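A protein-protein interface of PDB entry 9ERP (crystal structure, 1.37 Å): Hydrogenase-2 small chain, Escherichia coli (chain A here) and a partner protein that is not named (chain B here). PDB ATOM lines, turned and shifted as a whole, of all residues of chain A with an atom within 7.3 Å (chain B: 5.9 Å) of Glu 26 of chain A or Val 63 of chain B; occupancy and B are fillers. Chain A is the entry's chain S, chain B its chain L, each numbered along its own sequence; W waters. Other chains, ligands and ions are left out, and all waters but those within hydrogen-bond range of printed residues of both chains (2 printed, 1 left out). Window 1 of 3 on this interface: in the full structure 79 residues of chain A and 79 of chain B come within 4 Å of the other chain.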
ATOM      1  N   TRP A  15     -36.393 -23.078 -19.193  1.00  0.00           N
ATOM      2  CA  TRP A  15     -35.084 -23.729 -19.213  1.00  0.00           C
ATOM      3  C   TRP A  15     -35.114 -24.879 -18.215  1.00  0.00           C
ATOM      4  O   TRP A  15     -35.337 -24.658 -17.025  1.00  0.00           O
ATOM      5  CB  TRP A  15     -33.995 -22.724 -18.820  1.00  0.00           C
ATOM      6  CG  TRP A  15     -32.562 -23.229 -18.936  1.00  0.00           C
ATOM      7  CD1 TRP A  15     -32.025 -24.348 -18.368  1.00  0.00           C
ATOM      8  CD2 TRP A  15     -31.489 -22.581 -19.641  1.00  0.00           C
ATOM      9  NE1 TRP A  15     -30.676 -24.433 -18.678  1.00  0.00           N
ATOM     10  CE2 TRP A  15     -30.331 -23.361 -19.455  1.00  0.00           C
ATOM     11  CE3 TRP A  15     -31.409 -21.409 -20.390  1.00  0.00           C
ATOM     12  CZ2 TRP A  15     -29.099 -23.014 -20.020  1.00  0.00           C
ATOM     13  CZ3 TRP A  15     -30.184 -21.056 -20.942  1.00  0.00           C
ATOM     14  CH2 TRP A  15     -29.055 -21.863 -20.762  1.00  0.00           C
ATOM     15  N   CYS A  21     -24.018 -29.977 -15.931  1.00  0.00           N
ATOM     16  CA  CYS A  21     -23.001 -29.563 -14.968  1.00  0.00           C
ATOM     17  C   CYS A  21     -23.149 -28.097 -14.581  1.00  0.00           C
ATOM     18  O   CYS A  21     -22.422 -27.627 -13.691  1.00  0.00           O
ATOM     19  CB  CYS A  21     -21.606 -29.826 -15.526  1.00  0.00           C
ATOM     20  SG  CYS A  21     -21.022 -28.515 -16.643  1.00  0.00           S
ATOM     21  N   THR A  22     -24.089 -27.375 -15.220  1.00  0.00           N
ATOM     22  CA  THR A  22     -24.445 -25.971 -15.034  1.00  0.00           C
ATOM     23  C   THR A  22     -23.493 -25.068 -15.824  1.00  0.00           C
ATOM     24  O   THR A  22     -23.734 -23.870 -15.921  1.00  0.00           O
ATOM     25  CB  THR A  22     -24.600 -25.597 -13.563  1.00  0.00           C
ATOM     26  OG1 THR A  22     -25.434 -26.602 -12.943  1.00  0.00           O
ATOM     27  CG2 THR A  22     -25.271 -24.265 -13.382  1.00  0.00           C
ATOM     28  N   GLY A  23     -22.489 -25.622 -16.487  1.00  0.00           N
ATOM     29  CA  GLY A  23     -21.597 -24.791 -17.284  1.00  0.00           C
ATOM     30  C   GLY A  23     -22.286 -24.062 -18.420  1.00  0.00           C
ATOM     31  O   GLY A  23     -21.883 -22.958 -18.796  1.00  0.00           O
ATOM     32  N   CYS A  24     -23.348 -24.647 -18.970  1.00  0.00           N
ATOM     33  CA  CYS A  24     -24.061 -23.985 -20.061  1.00  0.00           C
ATOM     34  C   CYS A  24     -24.839 -22.773 -19.562  1.00  0.00           C
ATOM     35  O   CYS A  24     -24.822 -21.717 -20.201  1.00  0.00           O
ATOM     36  CB  CYS A  24     -24.964 -24.996 -20.792  1.00  0.00           C
ATOM     37  SG  CYS A  24     -24.079 -26.206 -21.818  1.00  0.00           S
ATOM     38  N   THR A  25     -25.487 -22.868 -18.395  1.00  0.00           N
ATOM     39  CA  THR A  25     -26.040 -21.674 -17.767  1.00  0.00           C
ATOM     40  C   THR A  25     -24.942 -20.677 -17.416  1.00  0.00           C
ATOM     41  O   THR A  25     -25.103 -19.460 -17.610  1.00  0.00           O
ATOM     42  CB  THR A  25     -26.815 -22.081 -16.503  1.00  0.00           C
ATOM     43  OG1 THR A  25     -28.015 -22.770 -16.880  1.00  0.00           O
ATOM     44  CG2 THR A  25     -27.180 -20.852 -15.667  1.00  0.00           C
ATOM     45  N   GLU A  26     -23.827 -21.175 -16.872  1.00  0.00           N
ATOM     46  CA  GLU A  26     -22.744 -20.285 -16.468  1.00  0.00           C
ATOM     47  C   GLU A  26     -22.182 -19.510 -17.638  1.00  0.00           C
ATOM     48  O   GLU A  26     -21.713 -18.388 -17.450  1.00  0.00           O
ATOM     49  CB  GLU A  26     -21.636 -21.098 -15.790  1.00  0.00           C
ATOM     50  CG  GLU A  26     -22.009 -21.453 -14.357  1.00  0.00           C
ATOM     51  CD  GLU A  26     -21.834 -20.353 -13.345  1.00  0.00           C
ATOM     52  OE1 GLU A  26     -21.461 -19.239 -13.707  1.00  0.00           O
ATOM     53  OE2 GLU A  26     -22.123 -20.600 -12.140  1.00  0.00           O
ATOM     54  N   SER A  27     -22.236 -20.067 -18.846  1.00  0.00           N
ATOM     55  CA  SER A  27     -21.770 -19.304 -19.998  1.00  0.00           C
ATOM     56  C   SER A  27     -22.475 -17.951 -20.088  1.00  0.00           C
ATOM     57  O   SER A  27     -21.850 -16.946 -20.477  1.00  0.00           O
ATOM     58  CB  SER A  27     -21.937 -20.106 -21.311  1.00  0.00           C
ATOM     59  OG  SER A  27     -23.280 -20.157 -21.768  1.00  0.00           O
ATOM     60  N   LEU A  28     -23.750 -17.905 -19.699  1.00  0.00           N
ATOM     61  CA  LEU A  28     -24.505 -16.665 -19.776  1.00  0.00           C
ATOM     62  C   LEU A  28     -23.912 -15.585 -18.895  1.00  0.00           C
ATOM     63  O   LEU A  28     -24.064 -14.405 -19.194  1.00  0.00           O
ATOM     64  CB  LEU A  28     -25.957 -16.895 -19.349  1.00  0.00           C
ATOM     65  CG  LEU A  28     -26.714 -17.950 -20.146  1.00  0.00           C
ATOM     66  CD1 LEU A  28     -28.140 -18.003 -19.635  1.00  0.00           C
ATOM     67  CD2 LEU A  28     -26.654 -17.646 -21.627  1.00  0.00           C
ATOM     68  N   LEU A  29     -23.251 -15.971 -17.798  1.00  0.00           N
ATOM     69  CA  LEU A  29     -22.669 -14.972 -16.901  1.00  0.00           C
ATOM     70  C   LEU A  29     -21.405 -14.329 -17.457  1.00  0.00           C
ATOM     71  O   LEU A  29     -20.964 -13.326 -16.892  1.00  0.00           O
ATOM     72  CB  LEU A  29     -22.394 -15.567 -15.499  1.00  0.00           C
ATOM     73  CG  LEU A  29     -23.591 -15.542 -14.526  1.00  0.00           C
ATOM     74  CD1 LEU A  29     -24.748 -16.347 -15.022  1.00  0.00           C
ATOM     75  CD2 LEU A  29     -23.155 -16.058 -13.158  1.00  0.00           C
ATOM     76  N   ARG A  30     -20.840 -14.862 -18.542  1.00  0.00           N
ATOM     77  CA  ARG A  30     -19.754 -14.218 -19.262  1.00  0.00           C
ATOM     78  C   ARG A  30     -20.239 -13.366 -20.429  1.00  0.00           C
ATOM     79  O   ARG A  30     -19.436 -12.607 -21.008  1.00  0.00           O
ATOM     80  CB  ARG A  30     -18.823 -15.290 -19.856  1.00  0.00           C
ATOM     81  CG  ARG A  30     -17.963 -16.015 -18.832  1.00  0.00           C
ATOM     82  CD  ARG A  30     -18.761 -16.998 -17.970  1.00  0.00           C
ATOM     83  NE  ARG A  30     -17.883 -17.937 -17.283  1.00  0.00           N
ATOM     84  CZ  ARG A  30     -18.199 -18.552 -16.150  1.00  0.00           C
ATOM     85  NH1 ARG A  30     -19.385 -18.395 -15.603  1.00  0.00           N
ATOM     86  NH2 ARG A  30     -17.321 -19.368 -15.575  1.00  0.00           N
ATOM     87  N   ALA A  31     -21.493 -13.514 -20.839  1.00  0.00           N
ATOM     88  CA  ALA A  31     -22.001 -12.827 -22.025  1.00  0.00           C
ATOM     89  C   ALA A  31     -22.033 -11.314 -21.855  1.00  0.00           C
ATOM     90  O   ALA A  31     -22.203 -10.789 -20.758  1.00  0.00           O
ATOM     91  CB  ALA A  31     -23.407 -13.322 -22.343  1.00  0.00           C
ATOM     92  N   HIS A  49     -36.153 -21.145 -14.470  1.00  0.00           N
ATOM     93  CA  HIS A  49     -34.730 -21.497 -14.467  1.00  0.00           C
ATOM     94  C   HIS A  49     -34.351 -21.755 -13.019  1.00  0.00           C
ATOM     95  O   HIS A  49     -34.298 -20.819 -12.220  1.00  0.00           O
ATOM     96  CB  HIS A  49     -33.839 -20.417 -15.059  1.00  0.00           C
ATOM     97  CG  HIS A  49     -32.481 -20.944 -15.419  1.00  0.00           C
ATOM     98  ND1 HIS A  49     -31.711 -21.660 -14.528  1.00  0.00           N
ATOM     99  CD2 HIS A  49     -31.790 -20.913 -16.584  1.00  0.00           C
ATOM    100  CE1 HIS A  49     -30.591 -22.037 -15.129  1.00  0.00           C
ATOM    101  NE2 HIS A  49     -30.616 -21.598 -16.380  1.00  0.00           N
ATOM    102  N   VAL A  51     -31.590 -22.351 -11.483  1.00  0.00           N
ATOM    103  CA  VAL A  51     -30.386 -21.788 -10.884  1.00  0.00           C
ATOM    104  C   VAL A  51     -30.636 -20.389 -10.338  1.00  0.00           C
ATOM    105  O   VAL A  51     -30.012 -19.983  -9.350  1.00  0.00           O
ATOM    106  CB  VAL A  51     -29.216 -21.802 -11.894  1.00  0.00           C
ATOM    107  CG1 VAL A  51     -27.981 -21.120 -11.308  1.00  0.00           C
ATOM    108  CG2 VAL A  51     -28.895 -23.235 -12.319  1.00  0.00           C
ATOM    109  N   ASP A  80     -30.246 -28.075 -21.100  1.00  0.00           N
ATOM    110  CA  ASP A  80     -28.846 -28.445 -20.975  1.00  0.00           C
ATOM    111  C   ASP A  80     -28.735 -29.776 -20.228  1.00  0.00           C
ATOM    112  O   ASP A  80     -29.608 -30.142 -19.436  1.00  0.00           O
ATOM    113  CB  ASP A  80     -27.967 -27.354 -20.332  1.00  0.00           C
ATOM    114  CG  ASP A  80     -28.423 -26.888 -18.951  1.00  0.00           C
ATOM    115  OD1 ASP A  80     -29.567 -27.108 -18.530  1.00  0.00           O
ATOM    116  OD2 ASP A  80     -27.583 -26.228 -18.277  1.00  0.00           O
ATOM    117  N   PRO A 154     -18.866 -25.469 -22.460  1.00  0.00           N
ATOM    118  CA  PRO A 154     -20.090 -24.998 -23.104  1.00  0.00           C
ATOM    119  C   PRO A 154     -19.796 -24.166 -24.343  1.00  0.00           C
ATOM    120  O   PRO A 154     -18.688 -23.688 -24.554  1.00  0.00           O
ATOM    121  CB  PRO A 154     -20.716 -24.117 -22.023  1.00  0.00           C
ATOM    122  CG  PRO A 154     -19.499 -23.482 -21.345  1.00  0.00           C
ATOM    123  CD  PRO A 154     -18.391 -24.523 -21.418  1.00  0.00           C
ATOM    124  N   PRO A 157     -21.598 -18.219 -25.202  1.00  0.00           N
ATOM    125  CA  PRO A 157     -23.016 -17.986 -24.919  1.00  0.00           C
ATOM    126  C   PRO A 157     -23.745 -17.269 -26.040  1.00  0.00           C
ATOM    127  O   PRO A 157     -24.965 -17.413 -26.144  1.00  0.00           O
ATOM    128  CB  PRO A 157     -22.996 -17.104 -23.664  1.00  0.00           C
ATOM    129  CG  PRO A 157     -21.608 -16.462 -23.659  1.00  0.00           C
ATOM    130  CD  PRO A 157     -20.717 -17.538 -24.230  1.00  0.00           C
ATOM    131  N   GLU B  14     -26.420 -25.268  -7.459  1.00  0.00           N
ATOM    132  CA  GLU B  14     -26.051 -26.028  -8.650  1.00  0.00           C
ATOM    133  C   GLU B  14     -26.655 -27.414  -8.541  1.00  0.00           C
ATOM    134  O   GLU B  14     -26.441 -28.121  -7.545  1.00  0.00           O
ATOM    135  CB  GLU B  14     -24.533 -26.120  -8.805  1.00  0.00           C
ATOM    136  CG  GLU B  14     -24.036 -26.765 -10.132  1.00  0.00           C
ATOM    137  CD  GLU B  14     -24.488 -28.193 -10.355  1.00  0.00           C
ATOM    138  OE1 GLU B  14     -24.555 -28.972  -9.390  1.00  0.00           O
ATOM    139  OE2 GLU B  14     -24.816 -28.573 -11.522  1.00  0.00           O
ATOM    140  N   CYS B  61     -18.473 -30.331 -12.931  1.00  0.00           N
ATOM    141  CA  CYS B  61     -19.208 -29.127 -12.567  1.00  0.00           C
ATOM    142  C   CYS B  61     -18.726 -27.907 -13.344  1.00  0.00           C
ATOM    143  O   CYS B  61     -17.522 -27.681 -13.489  1.00  0.00           O
ATOM    144  CB  CYS B  61     -19.075 -28.883 -11.065  1.00  0.00           C
ATOM    145  SG  CYS B  61     -20.072 -27.527 -10.443  1.00  0.00           S
ATOM    146  N   GLY B  62     -19.687 -27.104 -13.787  1.00  0.00           N
ATOM    147  CA  GLY B  62     -19.374 -25.867 -14.459  1.00  0.00           C
ATOM    148  C   GLY B  62     -19.553 -24.635 -13.619  1.00  0.00           C
ATOM    149  O   GLY B  62     -19.183 -23.537 -14.058  1.00  0.00           O
ATOM    150  N   VAL B  63     -20.159 -24.774 -12.434  1.00  0.00           N
ATOM    151  CA  VAL B  63     -20.133 -23.679 -11.462  1.00  0.00           C
ATOM    152  C   VAL B  63     -18.744 -23.587 -10.856  1.00  0.00           C
ATOM    153  O   VAL B  63     -18.030 -22.605 -11.052  1.00  0.00           O
ATOM    154  CB  VAL B  63     -21.197 -23.872 -10.375  1.00  0.00           C
ATOM    155  CG1 VAL B  63     -21.040 -22.787  -9.322  1.00  0.00           C
ATOM    156  CG2 VAL B  63     -22.596 -23.825 -10.964  1.00  0.00           C
ATOM    157  N   CYS B  64     -18.305 -24.663 -10.200  1.00  0.00           N
ATOM    158  CA  CYS B  64     -16.920 -24.767  -9.761  1.00  0.00           C
ATOM    159  C   CYS B  64     -16.044 -25.304 -10.891  1.00  0.00           C
ATOM    160  O   CYS B  64     -15.270 -26.259 -10.720  1.00  0.00           O
ATOM    161  CB  CYS B  64     -16.786 -25.561  -8.467  1.00  0.00           C
ATOM    162  SG  CYS B  64     -17.244 -27.295  -8.553  1.00  0.00           S
ATOM    163  N   THR B  65     -16.176 -24.714 -12.063  1.00  0.00           N
ATOM    164  CA  THR B  65     -15.216 -24.977 -13.125  1.00  0.00           C
ATOM    165  C   THR B  65     -13.813 -24.661 -12.609  1.00  0.00           C
ATOM    166  O   THR B  65     -13.635 -23.995 -11.595  1.00  0.00           O
ATOM    167  CB  THR B  65     -15.626 -24.233 -14.393  1.00  0.00           C
ATOM    168  OG1 THR B  65     -14.836 -24.700 -15.492  1.00  0.00           O
ATOM    169  CG2 THR B  65     -15.454 -22.737 -14.282  1.00  0.00           C
ATOM    170  N   HIS B  99     -11.248 -17.526 -10.284  1.00  0.00           N
ATOM    171  CA  HIS B  99     -12.475 -18.285 -10.388  1.00  0.00           C
ATOM    172  C   HIS B  99     -13.277 -18.209  -9.092  1.00  0.00           C
ATOM    173  O   HIS B  99     -14.500 -17.999  -9.097  1.00  0.00           O
ATOM    174  CB  HIS B  99     -12.236 -19.766 -10.686  1.00  0.00           C
ATOM    175  CG  HIS B  99     -13.505 -20.523 -10.508  1.00  0.00           C
ATOM    176  ND1 HIS B  99     -14.501 -20.504 -11.462  1.00  0.00           N
ATOM    177  CD2 HIS B  99     -14.027 -21.127  -9.419  1.00  0.00           C
ATOM    178  CE1 HIS B  99     -15.563 -21.119 -10.979  1.00  0.00           C
ATOM    179  NE2 HIS B  99     -15.297 -21.513  -9.747  1.00  0.00           N
ATOM    180  N   HIS B 102     -15.244 -14.982  -8.610  1.00  0.00           N
ATOM    181  CA  HIS B 102     -16.506 -15.089  -9.346  1.00  0.00           C
ATOM    182  C   HIS B 102     -17.506 -15.948  -8.607  1.00  0.00           C
ATOM    183  O   HIS B 102     -18.669 -15.579  -8.444  1.00  0.00           O
ATOM    184  CB  HIS B 102     -16.218 -15.669 -10.755  1.00  0.00           C
ATOM    185  CG  HIS B 102     -17.322 -16.540 -11.304  1.00  0.00           C
ATOM    186  ND1 HIS B 102     -18.447 -16.059 -11.935  1.00  0.00           N
ATOM    187  CD2 HIS B 102     -17.441 -17.891 -11.299  1.00  0.00           C
ATOM    188  CE1 HIS B 102     -19.229 -17.067 -12.268  1.00  0.00           C
ATOM    189  NE2 HIS B 102     -18.641 -18.191 -11.901  1.00  0.00           N
ATOM    190  N   ASP B 103     -17.065 -17.110  -8.157  1.00  0.00           N
ATOM    191  CA  ASP B 103     -17.965 -18.111  -7.593  1.00  0.00           C
ATOM    192  C   ASP B 103     -18.619 -17.570  -6.322  1.00  0.00           C
ATOM    193  O   ASP B 103     -19.850 -17.535  -6.200  1.00  0.00           O
ATOM    194  CB  ASP B 103     -17.115 -19.370  -7.355  1.00  0.00           C
ATOM    195  CG  ASP B 103     -17.916 -20.649  -7.272  1.00  0.00           C
ATOM    196  OD1 ASP B 103     -19.046 -20.622  -6.773  1.00  0.00           O
ATOM    197  OD2 ASP B 103     -17.340 -21.698  -7.640  1.00  0.00           O
ATOM    198  N   VAL B 106     -21.140 -14.632  -6.942  1.00  0.00           N
ATOM    199  CA  VAL B 106     -22.398 -15.125  -7.494  1.00  0.00           C
ATOM    200  C   VAL B 106     -23.198 -15.869  -6.433  1.00  0.00           C
ATOM    201  O   VAL B 106     -24.427 -15.746  -6.363  1.00  0.00           O
ATOM    202  CB  VAL B 106     -22.103 -15.993  -8.729  1.00  0.00           C
ATOM    203  CG1 VAL B 106     -23.335 -16.781  -9.161  1.00  0.00           C
ATOM    204  CG2 VAL B 106     -21.576 -15.092  -9.880  1.00  0.00           C
ATOM    205  N   LEU B 111     -27.337 -16.455  -6.012  1.00  0.00           N
ATOM    206  CA  LEU B 111     -27.879 -17.683  -5.428  1.00  0.00           C
ATOM    207  C   LEU B 111     -28.541 -17.438  -4.078  1.00  0.00           C
ATOM    208  O   LEU B 111     -29.602 -18.013  -3.826  1.00  0.00           O
ATOM    209  CB  LEU B 111     -26.825 -18.793  -5.344  1.00  0.00           C
ATOM    210  CG  LEU B 111     -26.103 -19.084  -6.676  1.00  0.00           C
ATOM    211  CD1 LEU B 111     -25.125 -20.222  -6.530  1.00  0.00           C
ATOM    212  CD2 LEU B 111     -27.142 -19.440  -7.744  1.00  0.00           C
ATOM    213  N   GLN B 198     -18.100 -10.074 -11.105  1.00  0.00           N
ATOM    214  CA  GLN B 198     -17.816 -11.476 -11.406  1.00  0.00           C
ATOM    215  C   GLN B 198     -17.401 -11.658 -12.857  1.00  0.00           C
ATOM    216  O   GLN B 198     -16.569 -12.530 -13.157  1.00  0.00           O
ATOM    217  CB  GLN B 198     -19.002 -12.368 -11.005  1.00  0.00           C
ATOM    218  CG  GLN B 198     -20.308 -12.216 -11.791  1.00  0.00           C
ATOM    219  CD  GLN B 198     -20.316 -12.923 -13.139  1.00  0.00           C
ATOM    220  OE1 GLN B 198     -19.735 -13.989 -13.282  1.00  0.00           O
ATOM    221  NE2 GLN B 198     -21.039 -12.367 -14.104  1.00  0.00           N
ATOM    222  N   ASN B 202     -13.851 -13.458 -14.172  1.00  0.00           N
ATOM    223  CA  ASN B 202     -13.724 -14.494 -15.181  1.00  0.00           C
ATOM    224  C   ASN B 202     -12.931 -14.064 -16.406  1.00  0.00           C
ATOM    225  O   ASN B 202     -12.431 -14.941 -17.114  1.00  0.00           O
ATOM    226  CB  ASN B 202     -15.078 -15.053 -15.539  1.00  0.00           C
ATOM    227  CG  ASN B 202     -15.480 -16.155 -14.556  1.00  0.00           C
ATOM    228  OD1 ASN B 202     -14.603 -16.793 -13.952  1.00  0.00           O
ATOM    229  ND2 ASN B 202     -16.743 -16.363 -14.409  1.00  0.00           N
ATOM    230  N   PRO B 213     -16.699 -20.837 -18.991  1.00  0.00           N
ATOM    231  CA  PRO B 213     -16.426 -22.076 -18.234  1.00  0.00           C
ATOM    232  C   PRO B 213     -15.546 -23.084 -18.977  1.00  0.00           C
ATOM    233  O   PRO B 213     -15.486 -23.142 -20.211  1.00  0.00           O
ATOM    234  CB  PRO B 213     -17.833 -22.656 -17.946  1.00  0.00           C
ATOM    235  CG  PRO B 213     -18.801 -21.521 -18.206  1.00  0.00           C
ATOM    236  CD  PRO B 213     -18.142 -20.685 -19.288  1.00  0.00           C
ATOM    237  N   ARG B 479     -16.141 -24.532  -2.244  1.00  0.00           N
ATOM    238  CA  ARG B 479     -17.053 -25.182  -1.314  1.00  0.00           C
ATOM    239  C   ARG B 479     -16.346 -26.090  -0.326  1.00  0.00           C
ATOM    240  O   ARG B 479     -17.020 -26.689   0.530  1.00  0.00           O
ATOM    241  CB  ARG B 479     -18.133 -25.933  -2.085  1.00  0.00           C
ATOM    242  CG  ARG B 479     -19.051 -24.978  -2.829  1.00  0.00           C
ATOM    243  CD  ARG B 479     -19.835 -25.599  -3.950  1.00  0.00           C
ATOM    244  NE  ARG B 479     -20.604 -24.588  -4.657  1.00  0.00           N
ATOM    245  CZ  ARG B 479     -20.055 -23.711  -5.497  1.00  0.00           C
ATOM    246  NH1 ARG B 479     -18.810 -23.841  -5.918  1.00  0.00           N
ATOM    247  NH2 ARG B 479     -20.775 -22.702  -5.944  1.00  0.00           N
ATOM    248  N   ASP B 544     -23.682 -23.497   0.154  1.00  0.00           N
ATOM    249  CA  ASP B 544     -23.392 -23.353  -1.290  1.00  0.00           C
ATOM    250  C   ASP B 544     -23.434 -24.728  -1.953  1.00  0.00           C
ATOM    251  O   ASP B 544     -22.432 -25.179  -2.543  1.00  0.00           O
ATOM    252  CB  ASP B 544     -22.042 -22.638  -1.422  1.00  0.00           C
ATOM    253  CG  ASP B 544     -21.671 -22.266  -2.841  1.00  0.00           C
ATOM    254  OD1 ASP B 544     -22.502 -22.341  -3.747  1.00  0.00           O
ATOM    255  OD2 ASP B 544     -20.509 -21.826  -2.987  1.00  0.00           O
ATOM    256  N   CYS B 546     -23.555 -27.828  -4.323  1.00  0.00           N
ATOM    257  CA  CYS B 546     -23.272 -28.141  -5.721  1.00  0.00           C
ATOM    258  C   CYS B 546     -23.504 -29.644  -5.849  1.00  0.00           C
ATOM    259  O   CYS B 546     -22.699 -30.463  -5.392  1.00  0.00           O
ATOM    260  CB  CYS B 546     -21.867 -27.759  -6.084  1.00  0.00           C
ATOM    261  SG  CYS B 546     -21.609 -27.991  -7.863  1.00  0.00           S
HETATM  262  O   HOH W   1     -21.123 -18.932 -10.434  1.00  0.00           O
HETATM  263  O   HOH W   2     -18.407 -14.604 -15.761  1.00  0.00           O
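Water W1 lies within hydrogen-bond range of the side-chain carboxylate (OE2) of Glu 26 of chain A (2.6 Å) and a ring nitrogen (NE2) of His 102 of chain B (3.0 Å).
Water W2 lies within hydrogen-bond range of ND2 of Asn 202 of chain B, OE1 of Gln 198 of chain B and O of Leu 29 of chain A.
Cys 61 of chain B touches Cys 21 of chain A.
O of Cys 21 of chain A touches N of Val 63 of chain B (3.9 Å).
Val 63 of chain B touches Thr 22 of chain A.
Val 63 of chain B touches Glu 26 of chain A (CG2 to OE2, 3.5 Å).
Glu 26 of chain A touches His 102 of chain B (OE1 to CE1, 3.4 Å).
Glu 26 of chain A touches Pro 213 of chain B (CB to CG, 3.7 Å).
Pro 213 of chain B touches Ser 27 of chain A.
NH1 of Arg 30 of chain A touches CE1 of His 102 of chain B, at 3.6 Å.
Arg 30 of chain A touches Pro 213 of chain B.
Pro 154 of chain A touches Pro 213 of chain B.
The side-chain sulfur (SG) of Cys 21 of chain A lies close to the backbone NH (N) of Gly 23 of chain A (3.2 Å).
NH1 of Arg 30 of chain A is in salt-bridge range of OE1 of Glu 26 of chain A (2.9 Å).
ND1 of His 49 of chain A is in hydrogen-bond range of N of Val 51 of chain A (3.1 Å).
The side-chain sulfur (SG) of Cys 61 of chain B sits close to the backbone NH (N) of Val 63 of chain B, at 3.4 Å.
The backbone carbonyl oxygen (O) of Val 63 of chain B sits close to a ring nitrogen (NE2) of His 99 of chain B (3.2 Å).
O of Val 106 of chain B lies within hydrogen-bond range of N of Leu 111 of chain B (3.0 Å).
Hydrophobic or aromatic side chains of chain A that line the printed part of chain B: Leu 29 and Pro 154.
Along chain A the printed residues that touch a printed residue of chain B span positions 21 to 154.
Of the 17 printed residues of chain B, 10 touch a printed residue of chain A.
Hydrophobic or aromatic side chains of chain B within 4 Å of the printed part of chain A: Val 63, His 102, Val 106, Leu 111 and Pro 213.
Along chain B the printed residues that touch a printed residue of chain A span positions 14 to 213.
Among the printed residues, 20 pairs touch across the chains.
Among the printed residues, no Asp or Glu carboxylate lies within 4 Å of a Lys or Arg side-chain nitrogen of the other chain.
N of Gly 62 of chain B lies within hydrogen-bond range of O of Cys 21 of chain A (2.8 Å).
The side-chain carboxylate of Glu 14 of chain B lies within hydrogen-bond range of the side-chain hydroxyl of Thr 22 of chain A, at 2.5 Å.
O of Leu 29 of chain A lies within hydrogen-bond range of NE2 of Gln 198 of chain B (2.9 Å).
The guanidinium group (NH2) of Arg 30 of chain A sits close to the side-chain amide nitrogen (ND2) of Asn 202 of chain B (3.3 Å).
OE2 of Glu 14 of chain B lies close to O of Cys 21 of chain A (3.4 Å).
Of chain B, only Gly 62, Val 63, His 102 and Pro 213 come within 4 Å of Glu 26 of chain A.
Of the printed residues of chain A, Val 63 of chain B touches Cys 21, Thr 22 and Glu 26.
Of the printed residues of chain B, Ser 27 of chain A touches Pro 213 (3.8 Å).
Of the printed residues of chain A, Cys 61 of chain B touches Cys 21.
Printed residues of chain A within 4 Å of Glu 14 of chain B: Cys 21 (3.4 Å) and Thr 22 (2.5 Å).
Of the printed residues of chain B, Cys 21 of chain A touches Glu 14 (3.4 Å), Cys 61 (3.7 Å), Gly 62 (2.8 Å) and Val 63 (3.9 Å).
Printed residues of chain B within 4 Å of Thr 22 of chain A: Glu 14 and Val 63.
The nearest residue of chain B that does not touch Glu 26 of chain A is Val 106 of chain B (5.0 Å).
The nearest residue of chain A that does not touch Val 63 of chain B is Gly 23 of chain A (4.8 Å).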
